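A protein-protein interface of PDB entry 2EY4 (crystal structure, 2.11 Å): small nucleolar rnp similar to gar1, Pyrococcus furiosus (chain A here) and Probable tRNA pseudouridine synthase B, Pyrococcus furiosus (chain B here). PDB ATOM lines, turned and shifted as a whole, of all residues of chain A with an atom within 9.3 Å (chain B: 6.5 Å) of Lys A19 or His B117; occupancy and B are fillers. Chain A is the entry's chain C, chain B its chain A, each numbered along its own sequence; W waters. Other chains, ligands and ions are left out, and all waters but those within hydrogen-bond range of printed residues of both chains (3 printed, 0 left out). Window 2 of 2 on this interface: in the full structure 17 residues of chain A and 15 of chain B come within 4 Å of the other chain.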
ATOM      1  N   HIS A  16      15.571  25.455 -31.431  1.00  0.00           N
ATOM      2  CA  HIS A  16      15.663  26.201 -30.183  1.00  0.00           C
ATOM      3  C   HIS A  16      16.761  27.245 -30.222  1.00  0.00           C
ATOM      4  O   HIS A  16      17.521  27.345 -31.190  1.00  0.00           O
ATOM      5  CB  HIS A  16      15.950  25.245 -29.028  1.00  0.00           C
ATOM      6  CG  HIS A  16      17.105  24.324 -29.287  1.00  0.00           C
ATOM      7  ND1 HIS A  16      16.940  23.012 -29.676  1.00  0.00           N
ATOM      8  CD2 HIS A  16      18.442  24.541 -29.253  1.00  0.00           C
ATOM      9  CE1 HIS A  16      18.125  22.459 -29.871  1.00  0.00           C
ATOM     10  NE2 HIS A  16      19.052  23.365 -29.622  1.00  0.00           N
ATOM     11  N   TYR A  17      16.837  28.016 -29.148  1.00  0.00           N
ATOM     12  CA  TYR A  17      17.860  29.034 -29.007  1.00  0.00           C
ATOM     13  C   TYR A  17      18.835  28.521 -27.955  1.00  0.00           C
ATOM     14  O   TYR A  17      18.646  28.752 -26.762  1.00  0.00           O
ATOM     15  CB  TYR A  17      17.253  30.347 -28.533  1.00  0.00           C
ATOM     16  CG  TYR A  17      18.277  31.433 -28.359  1.00  0.00           C
ATOM     17  CD1 TYR A  17      19.041  31.868 -29.442  1.00  0.00           C
ATOM     18  CD2 TYR A  17      18.490  32.024 -27.120  1.00  0.00           C
ATOM     19  CE1 TYR A  17      19.994  32.868 -29.293  1.00  0.00           C
ATOM     20  CE2 TYR A  17      19.445  33.029 -26.961  1.00  0.00           C
ATOM     21  CZ  TYR A  17      20.190  33.446 -28.049  1.00  0.00           C
ATOM     22  OH  TYR A  17      21.120  34.448 -27.910  1.00  0.00           O
ATOM     23  N   ALA A  18      19.865  27.810 -28.405  1.00  0.00           N
ATOM     24  CA  ALA A  18      20.864  27.246 -27.504  1.00  0.00           C
ATOM     25  C   ALA A  18      21.329  28.271 -26.474  1.00  0.00           C
ATOM     26  O   ALA A  18      21.588  29.426 -26.806  1.00  0.00           O
ATOM     27  CB  ALA A  18      22.051  26.725 -28.302  1.00  0.00           C
ATOM     28  N   LYS A  19      21.437  27.836 -25.222  1.00  0.00           N
ATOM     29  CA  LYS A  19      21.850  28.713 -24.132  1.00  0.00           C
ATOM     30  C   LYS A  19      23.145  29.462 -24.417  1.00  0.00           C
ATOM     31  O   LYS A  19      23.367  30.551 -23.891  1.00  0.00           O
ATOM     32  CB  LYS A  19      21.986  27.904 -22.838  1.00  0.00           C
ATOM     33  CG  LYS A  19      22.468  28.712 -21.641  1.00  0.00           C
ATOM     34  CD  LYS A  19      21.953  28.133 -20.327  1.00  0.00           C
ATOM     35  CE  LYS A  19      22.319  26.667 -20.157  1.00  0.00           C
ATOM     36  NZ  LYS A  19      21.689  26.090 -18.938  1.00  0.00           N
ATOM     37  N   GLN A  20      23.994  28.883 -25.258  1.00  0.00           N
ATOM     38  CA  GLN A  20      25.264  29.509 -25.593  1.00  0.00           C
ATOM     39  C   GLN A  20      25.155  30.646 -26.607  1.00  0.00           C
ATOM     40  O   GLN A  20      26.165  31.224 -27.009  1.00  0.00           O
ATOM     41  CB  GLN A  20      26.242  28.443 -26.078  1.00  0.00           C
ATOM     42  CG  GLN A  20      26.638  27.477 -24.978  1.00  0.00           C
ATOM     43  CD  GLN A  20      27.471  26.333 -25.487  1.00  0.00           C
ATOM     44  OE1 GLN A  20      26.996  25.501 -26.255  1.00  0.00           O
ATOM     45  NE2 GLN A  20      28.726  26.284 -25.066  1.00  0.00           N
ATOM     46  N   GLY A  21      23.933  30.958 -27.027  1.00  0.00           N
ATOM     47  CA  GLY A  21      23.735  32.060 -27.954  1.00  0.00           C
ATOM     48  C   GLY A  21      23.666  31.795 -29.448  1.00  0.00           C
ATOM     49  O   GLY A  21      24.171  32.596 -30.233  1.00  0.00           O
ATOM     50  N   PHE A  22      23.052  30.691 -29.855  1.00  0.00           N
ATOM     51  CA  PHE A  22      22.929  30.395 -31.275  1.00  0.00           C
ATOM     52  C   PHE A  22      21.572  29.799 -31.592  1.00  0.00           C
ATOM     53  O   PHE A  22      20.967  29.134 -30.756  1.00  0.00           O
ATOM     54  CB  PHE A  22      24.002  29.403 -31.740  1.00  0.00           C
ATOM     55  CG  PHE A  22      25.397  29.916 -31.617  1.00  0.00           C
ATOM     56  CD1 PHE A  22      26.079  29.835 -30.407  1.00  0.00           C
ATOM     57  CD2 PHE A  22      26.029  30.501 -32.708  1.00  0.00           C
ATOM     58  CE1 PHE A  22      27.374  30.334 -30.288  1.00  0.00           C
ATOM     59  CE2 PHE A  22      27.316  31.000 -32.599  1.00  0.00           C
ATOM     60  CZ  PHE A  22      27.997  30.919 -31.386  1.00  0.00           C
ATOM     61  N   LEU A  23      21.091  30.052 -32.802  1.00  0.00           N
ATOM     62  CA  LEU A  23      19.832  29.478 -33.237  1.00  0.00           C
ATOM     63  C   LEU A  23      20.208  28.169 -33.923  1.00  0.00           C
ATOM     64  O   LEU A  23      21.033  28.150 -34.840  1.00  0.00           O
ATOM     65  CB  LEU A  23      19.121  30.408 -34.222  1.00  0.00           C
ATOM     66  CG  LEU A  23      18.579  31.728 -33.667  1.00  0.00           C
ATOM     67  CD1 LEU A  23      17.851  32.476 -34.771  1.00  0.00           C
ATOM     68  CD2 LEU A  23      17.634  31.454 -32.512  1.00  0.00           C
ATOM     69  N   ILE A  24      19.621  27.073 -33.460  1.00  0.00           N
ATOM     70  CA  ILE A  24      19.905  25.765 -34.029  1.00  0.00           C
ATOM     71  C   ILE A  24      18.769  25.296 -34.928  1.00  0.00           C
ATOM     72  O   ILE A  24      17.601  25.309 -34.546  1.00  0.00           O
ATOM     73  CB  ILE A  24      20.157  24.700 -32.927  1.00  0.00           C
ATOM     74  CG1 ILE A  24      21.509  24.945 -32.256  1.00  0.00           C
ATOM     75  CG2 ILE A  24      20.177  23.304 -33.537  1.00  0.00           C
ATOM     76  CD1 ILE A  24      21.644  26.283 -31.583  1.00  0.00           C
ATOM     77  N   GLU A  70      15.147  34.140 -29.980  1.00  0.00           N
ATOM     78  CA  GLU A  70      14.215  33.329 -29.209  1.00  0.00           C
ATOM     79  C   GLU A  70      12.790  33.383 -29.749  1.00  0.00           C
ATOM     80  O   GLU A  70      11.986  32.491 -29.479  1.00  0.00           O
ATOM     81  CB  GLU A  70      14.231  33.774 -27.743  1.00  0.00           C
ATOM     82  CG  GLU A  70      15.597  33.645 -27.083  1.00  0.00           C
ATOM     83  CD  GLU A  70      15.628  34.203 -25.675  1.00  0.00           C
ATOM     84  OE1 GLU A  70      15.438  35.428 -25.516  1.00  0.00           O
ATOM     85  OE2 GLU A  70      15.845  33.416 -24.726  1.00  0.00           O
ATOM     86  N   HIS B 115      30.076  17.235 -19.687  1.00  0.00           N
ATOM     87  CA  HIS B 115      29.341  17.918 -18.640  1.00  0.00           C
ATOM     88  C   HIS B 115      28.294  18.831 -19.252  1.00  0.00           C
ATOM     89  O   HIS B 115      28.625  19.865 -19.826  1.00  0.00           O
ATOM     90  CB  HIS B 115      30.261  18.749 -17.751  1.00  0.00           C
ATOM     91  CG  HIS B 115      29.551  19.344 -16.574  1.00  0.00           C
ATOM     92  ND1 HIS B 115      29.067  18.576 -15.535  1.00  0.00           N
ATOM     93  CD2 HIS B 115      29.157  20.615 -16.317  1.00  0.00           C
ATOM     94  CE1 HIS B 115      28.401  19.348 -14.694  1.00  0.00           C
ATOM     95  NE2 HIS B 115      28.441  20.588 -15.144  1.00  0.00           N
ATOM     96  N   LEU B 116      27.028  18.450 -19.120  1.00  0.00           N
ATOM     97  CA  LEU B 116      25.943  19.254 -19.671  1.00  0.00           C
ATOM     98  C   LEU B 116      25.729  20.505 -18.821  1.00  0.00           C
ATOM     99  O   LEU B 116      25.968  20.491 -17.616  1.00  0.00           O
ATOM    100  CB  LEU B 116      24.657  18.424 -19.732  1.00  0.00           C
ATOM    101  CG  LEU B 116      24.714  17.185 -20.628  1.00  0.00           C
ATOM    102  CD1 LEU B 116      23.429  16.383 -20.483  1.00  0.00           C
ATOM    103  CD2 LEU B 116      24.916  17.608 -22.075  1.00  0.00           C
ATOM    104  N   HIS B 117      25.290  21.589 -19.454  1.00  0.00           N
ATOM    105  CA  HIS B 117      25.045  22.842 -18.738  1.00  0.00           C
ATOM    106  C   HIS B 117      23.583  22.966 -18.315  1.00  0.00           C
ATOM    107  O   HIS B 117      23.162  24.001 -17.805  1.00  0.00           O
ATOM    108  CB  HIS B 117      25.410  24.034 -19.613  1.00  0.00           C
ATOM    109  CG  HIS B 117      26.834  24.036 -20.071  1.00  0.00           C
ATOM    110  ND1 HIS B 117      27.789  23.205 -19.531  1.00  0.00           N
ATOM    111  CD2 HIS B 117      27.472  24.799 -20.990  1.00  0.00           C
ATOM    112  CE1 HIS B 117      28.957  23.456 -20.095  1.00  0.00           C
ATOM    113  NE2 HIS B 117      28.793  24.418 -20.983  1.00  0.00           N
ATOM    114  N   GLY B 118      22.813  21.910 -18.534  1.00  0.00           N
ATOM    115  CA  GLY B 118      21.415  21.941 -18.163  1.00  0.00           C
ATOM    116  C   GLY B 118      20.879  20.547 -17.943  1.00  0.00           C
ATOM    117  O   GLY B 118      21.566  19.560 -18.202  1.00  0.00           O
ATOM    118  N   ASP B 119      19.643  20.456 -17.479  1.00  0.00           N
ATOM    119  CA  ASP B 119      19.040  19.161 -17.223  1.00  0.00           C
ATOM    120  C   ASP B 119      18.260  18.682 -18.434  1.00  0.00           C
ATOM    121  O   ASP B 119      17.324  19.336 -18.887  1.00  0.00           O
ATOM    122  CB  ASP B 119      18.159  19.256 -15.983  1.00  0.00           C
ATOM    123  CG  ASP B 119      18.924  19.805 -14.789  1.00  0.00           C
ATOM    124  OD1 ASP B 119      19.969  19.214 -14.435  1.00  0.00           O
ATOM    125  OD2 ASP B 119      18.492  20.829 -14.223  1.00  0.00           O
ATOM    126  N   ARG B 166      24.471  15.903 -14.431  1.00  0.00           N
ATOM    127  CA  ARG B 166      24.644  16.404 -15.782  1.00  0.00           C
ATOM    128  C   ARG B 166      25.910  15.834 -16.409  1.00  0.00           C
ATOM    129  O   ARG B 166      26.304  16.244 -17.501  1.00  0.00           O
ATOM    130  CB  ARG B 166      24.716  17.925 -15.771  1.00  0.00           C
ATOM    131  CG  ARG B 166      23.423  18.569 -15.360  1.00  0.00           C
ATOM    132  CD  ARG B 166      23.585  20.058 -15.140  1.00  0.00           C
ATOM    133  NE  ARG B 166      22.307  20.660 -14.780  1.00  0.00           N
ATOM    134  CZ  ARG B 166      22.167  21.896 -14.326  1.00  0.00           C
ATOM    135  NH1 ARG B 166      23.234  22.670 -14.174  1.00  0.00           N
ATOM    136  NH2 ARG B 166      20.958  22.349 -14.014  1.00  0.00           N
ATOM    137  N   LEU B 189      25.147  21.836 -28.275  1.00  0.00           N
ATOM    138  CA  LEU B 189      24.327  22.728 -29.077  1.00  0.00           C
ATOM    139  C   LEU B 189      23.097  21.977 -29.541  1.00  0.00           C
ATOM    140  O   LEU B 189      21.982  22.493 -29.467  1.00  0.00           O
ATOM    141  CB  LEU B 189      25.111  23.240 -30.286  1.00  0.00           C
ATOM    142  CG  LEU B 189      26.233  24.245 -30.009  1.00  0.00           C
ATOM    143  CD1 LEU B 189      26.911  24.622 -31.322  1.00  0.00           C
ATOM    144  CD2 LEU B 189      25.663  25.492 -29.336  1.00  0.00           C
ATOM    145  N   GLY B 192      20.722  21.935 -27.031  1.00  0.00           N
ATOM    146  CA  GLY B 192      20.337  23.264 -26.598  1.00  0.00           C
ATOM    147  C   GLY B 192      20.961  23.809 -25.328  1.00  0.00           C
ATOM    148  O   GLY B 192      21.371  24.970 -25.301  1.00  0.00           O
ATOM    149  N   VAL B 193      21.044  22.996 -24.278  1.00  0.00           N
ATOM    150  CA  VAL B 193      21.609  23.465 -23.009  1.00  0.00           C
ATOM    151  C   VAL B 193      23.110  23.729 -23.002  1.00  0.00           C
ATOM    152  O   VAL B 193      23.607  24.481 -22.155  1.00  0.00           O
ATOM    153  CB  VAL B 193      21.312  22.486 -21.845  1.00  0.00           C
ATOM    154  CG1 VAL B 193      19.814  22.367 -21.630  1.00  0.00           C
ATOM    155  CG2 VAL B 193      21.930  21.126 -22.136  1.00  0.00           C
ATOM    156  N   GLY B 194      23.830  23.101 -23.927  1.00  0.00           N
ATOM    157  CA  GLY B 194      25.268  23.289 -23.983  1.00  0.00           C
ATOM    158  C   GLY B 194      26.018  22.281 -23.129  1.00  0.00           C
ATOM    159  O   GLY B 194      25.461  21.693 -22.201  1.00  0.00           O
ATOM    160  N   ALA B 195      27.294  22.083 -23.434  1.00  0.00           N
ATOM    161  CA  ALA B 195      28.106  21.128 -22.698  1.00  0.00           C
ATOM    162  C   ALA B 195      29.569  21.328 -23.047  1.00  0.00           C
ATOM    163  O   ALA B 195      29.897  22.024 -24.009  1.00  0.00           O
ATOM    164  CB  ALA B 195      27.678  19.711 -23.055  1.00  0.00           C
ATOM    165  N   HIS B 196      30.447  20.733 -22.248  1.00  0.00           N
ATOM    166  CA  HIS B 196      31.876  20.805 -22.510  1.00  0.00           C
ATOM    167  C   HIS B 196      32.521  19.508 -22.030  1.00  0.00           C
ATOM    168  O   HIS B 196      31.956  18.787 -21.200  1.00  0.00           O
ATOM    169  CB  HIS B 196      32.515  21.999 -21.800  1.00  0.00           C
ATOM    170  CG  HIS B 196      32.598  21.843 -20.316  1.00  0.00           C
ATOM    171  ND1 HIS B 196      31.513  22.025 -19.485  1.00  0.00           N
ATOM    172  CD2 HIS B 196      33.632  21.496 -19.515  1.00  0.00           C
ATOM    173  CE1 HIS B 196      31.878  21.796 -18.237  1.00  0.00           C
ATOM    174  NE2 HIS B 196      33.159  21.474 -18.227  1.00  0.00           N
HETATM  175  O   HOH W   1      31.145  24.034 -25.070  1.00  0.00           O
HETATM  176  O   HOH W   2      27.993  23.206 -26.207  1.00  0.00           O
HETATM  177  O   HOH W   3      24.158  26.082 -25.912  1.00  0.00           O
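O of His B117 is in hydrogen-bond range of NZ of Lys A19. The backbone NH of Lys A19 sits at hydrogen-bond distance from the backbone carbonyl oxygen of Gly B192, 2.9 Å away. O of Leu B189 sits at hydrogen-bond distance from NE2 of His A16 (3.1 Å). A ring nitrogen (NE2) of His A16 lies close to the backbone NH of Gly B192 (3.4 Å).
The backbone NH (N) of His B117 lies within hydrogen-bond range of the backbone carbonyl oxygen (O) of Gly B194 (2.8 Å). O of His B115 is in hydrogen-bond range of ND1 of His B117, 3.5 Å away. The backbone carbonyl oxygen of His A16 lies within hydrogen-bond range of the backbone NH of Ile A24, at 3.1 Å.
Among the printed residues, merely in contact across the chains: Ala A18 with Gly B192 (3.2 Å), Lys A19 with Val B193 (3.2 Å), Gln A20 with Leu B189 (3.4 Å), Gln A20 with Gly B194 (3.6 Å), Ile A24 with Leu B189 (3.7 Å) and Ala A18 with Leu B189 (3.95 Å).
Printed residues of chain B within 4 Å of His A16: Leu B189 (3.1 Å) and Gly B192 (3.3 Å). Lys A19 touches three residues of chain B. Of the printed residues of chain B, Ile A24 touches Leu B189. Of chain A, only Lys A19 comes within 4 Å of His B117. No residue of chain A comes within 4 Å of Gly B118. Val B193 touches just one residue of chain A: Lys A19. No residue of chain A comes within 4 Å of Ala B195. The nearest residue of chain A that does not touch His B117 is Gln A20 (4.5 Å).
Of the 12 printed residues of chain B, 5 touch a printed residue of chain A. Printed residues of chain B that touch a printed residue of chain A: His B117, Leu B189, Gly B192, Val B193 and Gly B194. Hydrophobic or aromatic side chains of chain B that line the printed part of chain A: Leu B189. Printed residues of chain A that touch a printed residue of chain B: His A16, Ala A18, Lys A19, Gln A20 and Ile A24. Among the printed residues, no Asp or Glu carboxylate lies within 4 Å of a Lys or Arg side-chain nitrogen of the other chain.
Water W2 lies within hydrogen-bond range of OE1 of Gln A20 (2.5 Å) and N of Ala B195 (3.1 Å). Water W1 lies within hydrogen-bond range of O of Ala B195 and NE2 of Gln A20. Water W3 lies within hydrogen-bond range of N of Gln A20 (2.9 Å), O of Gly B192 (3.1 Å) and N of Lys A19 (3.3 Å).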
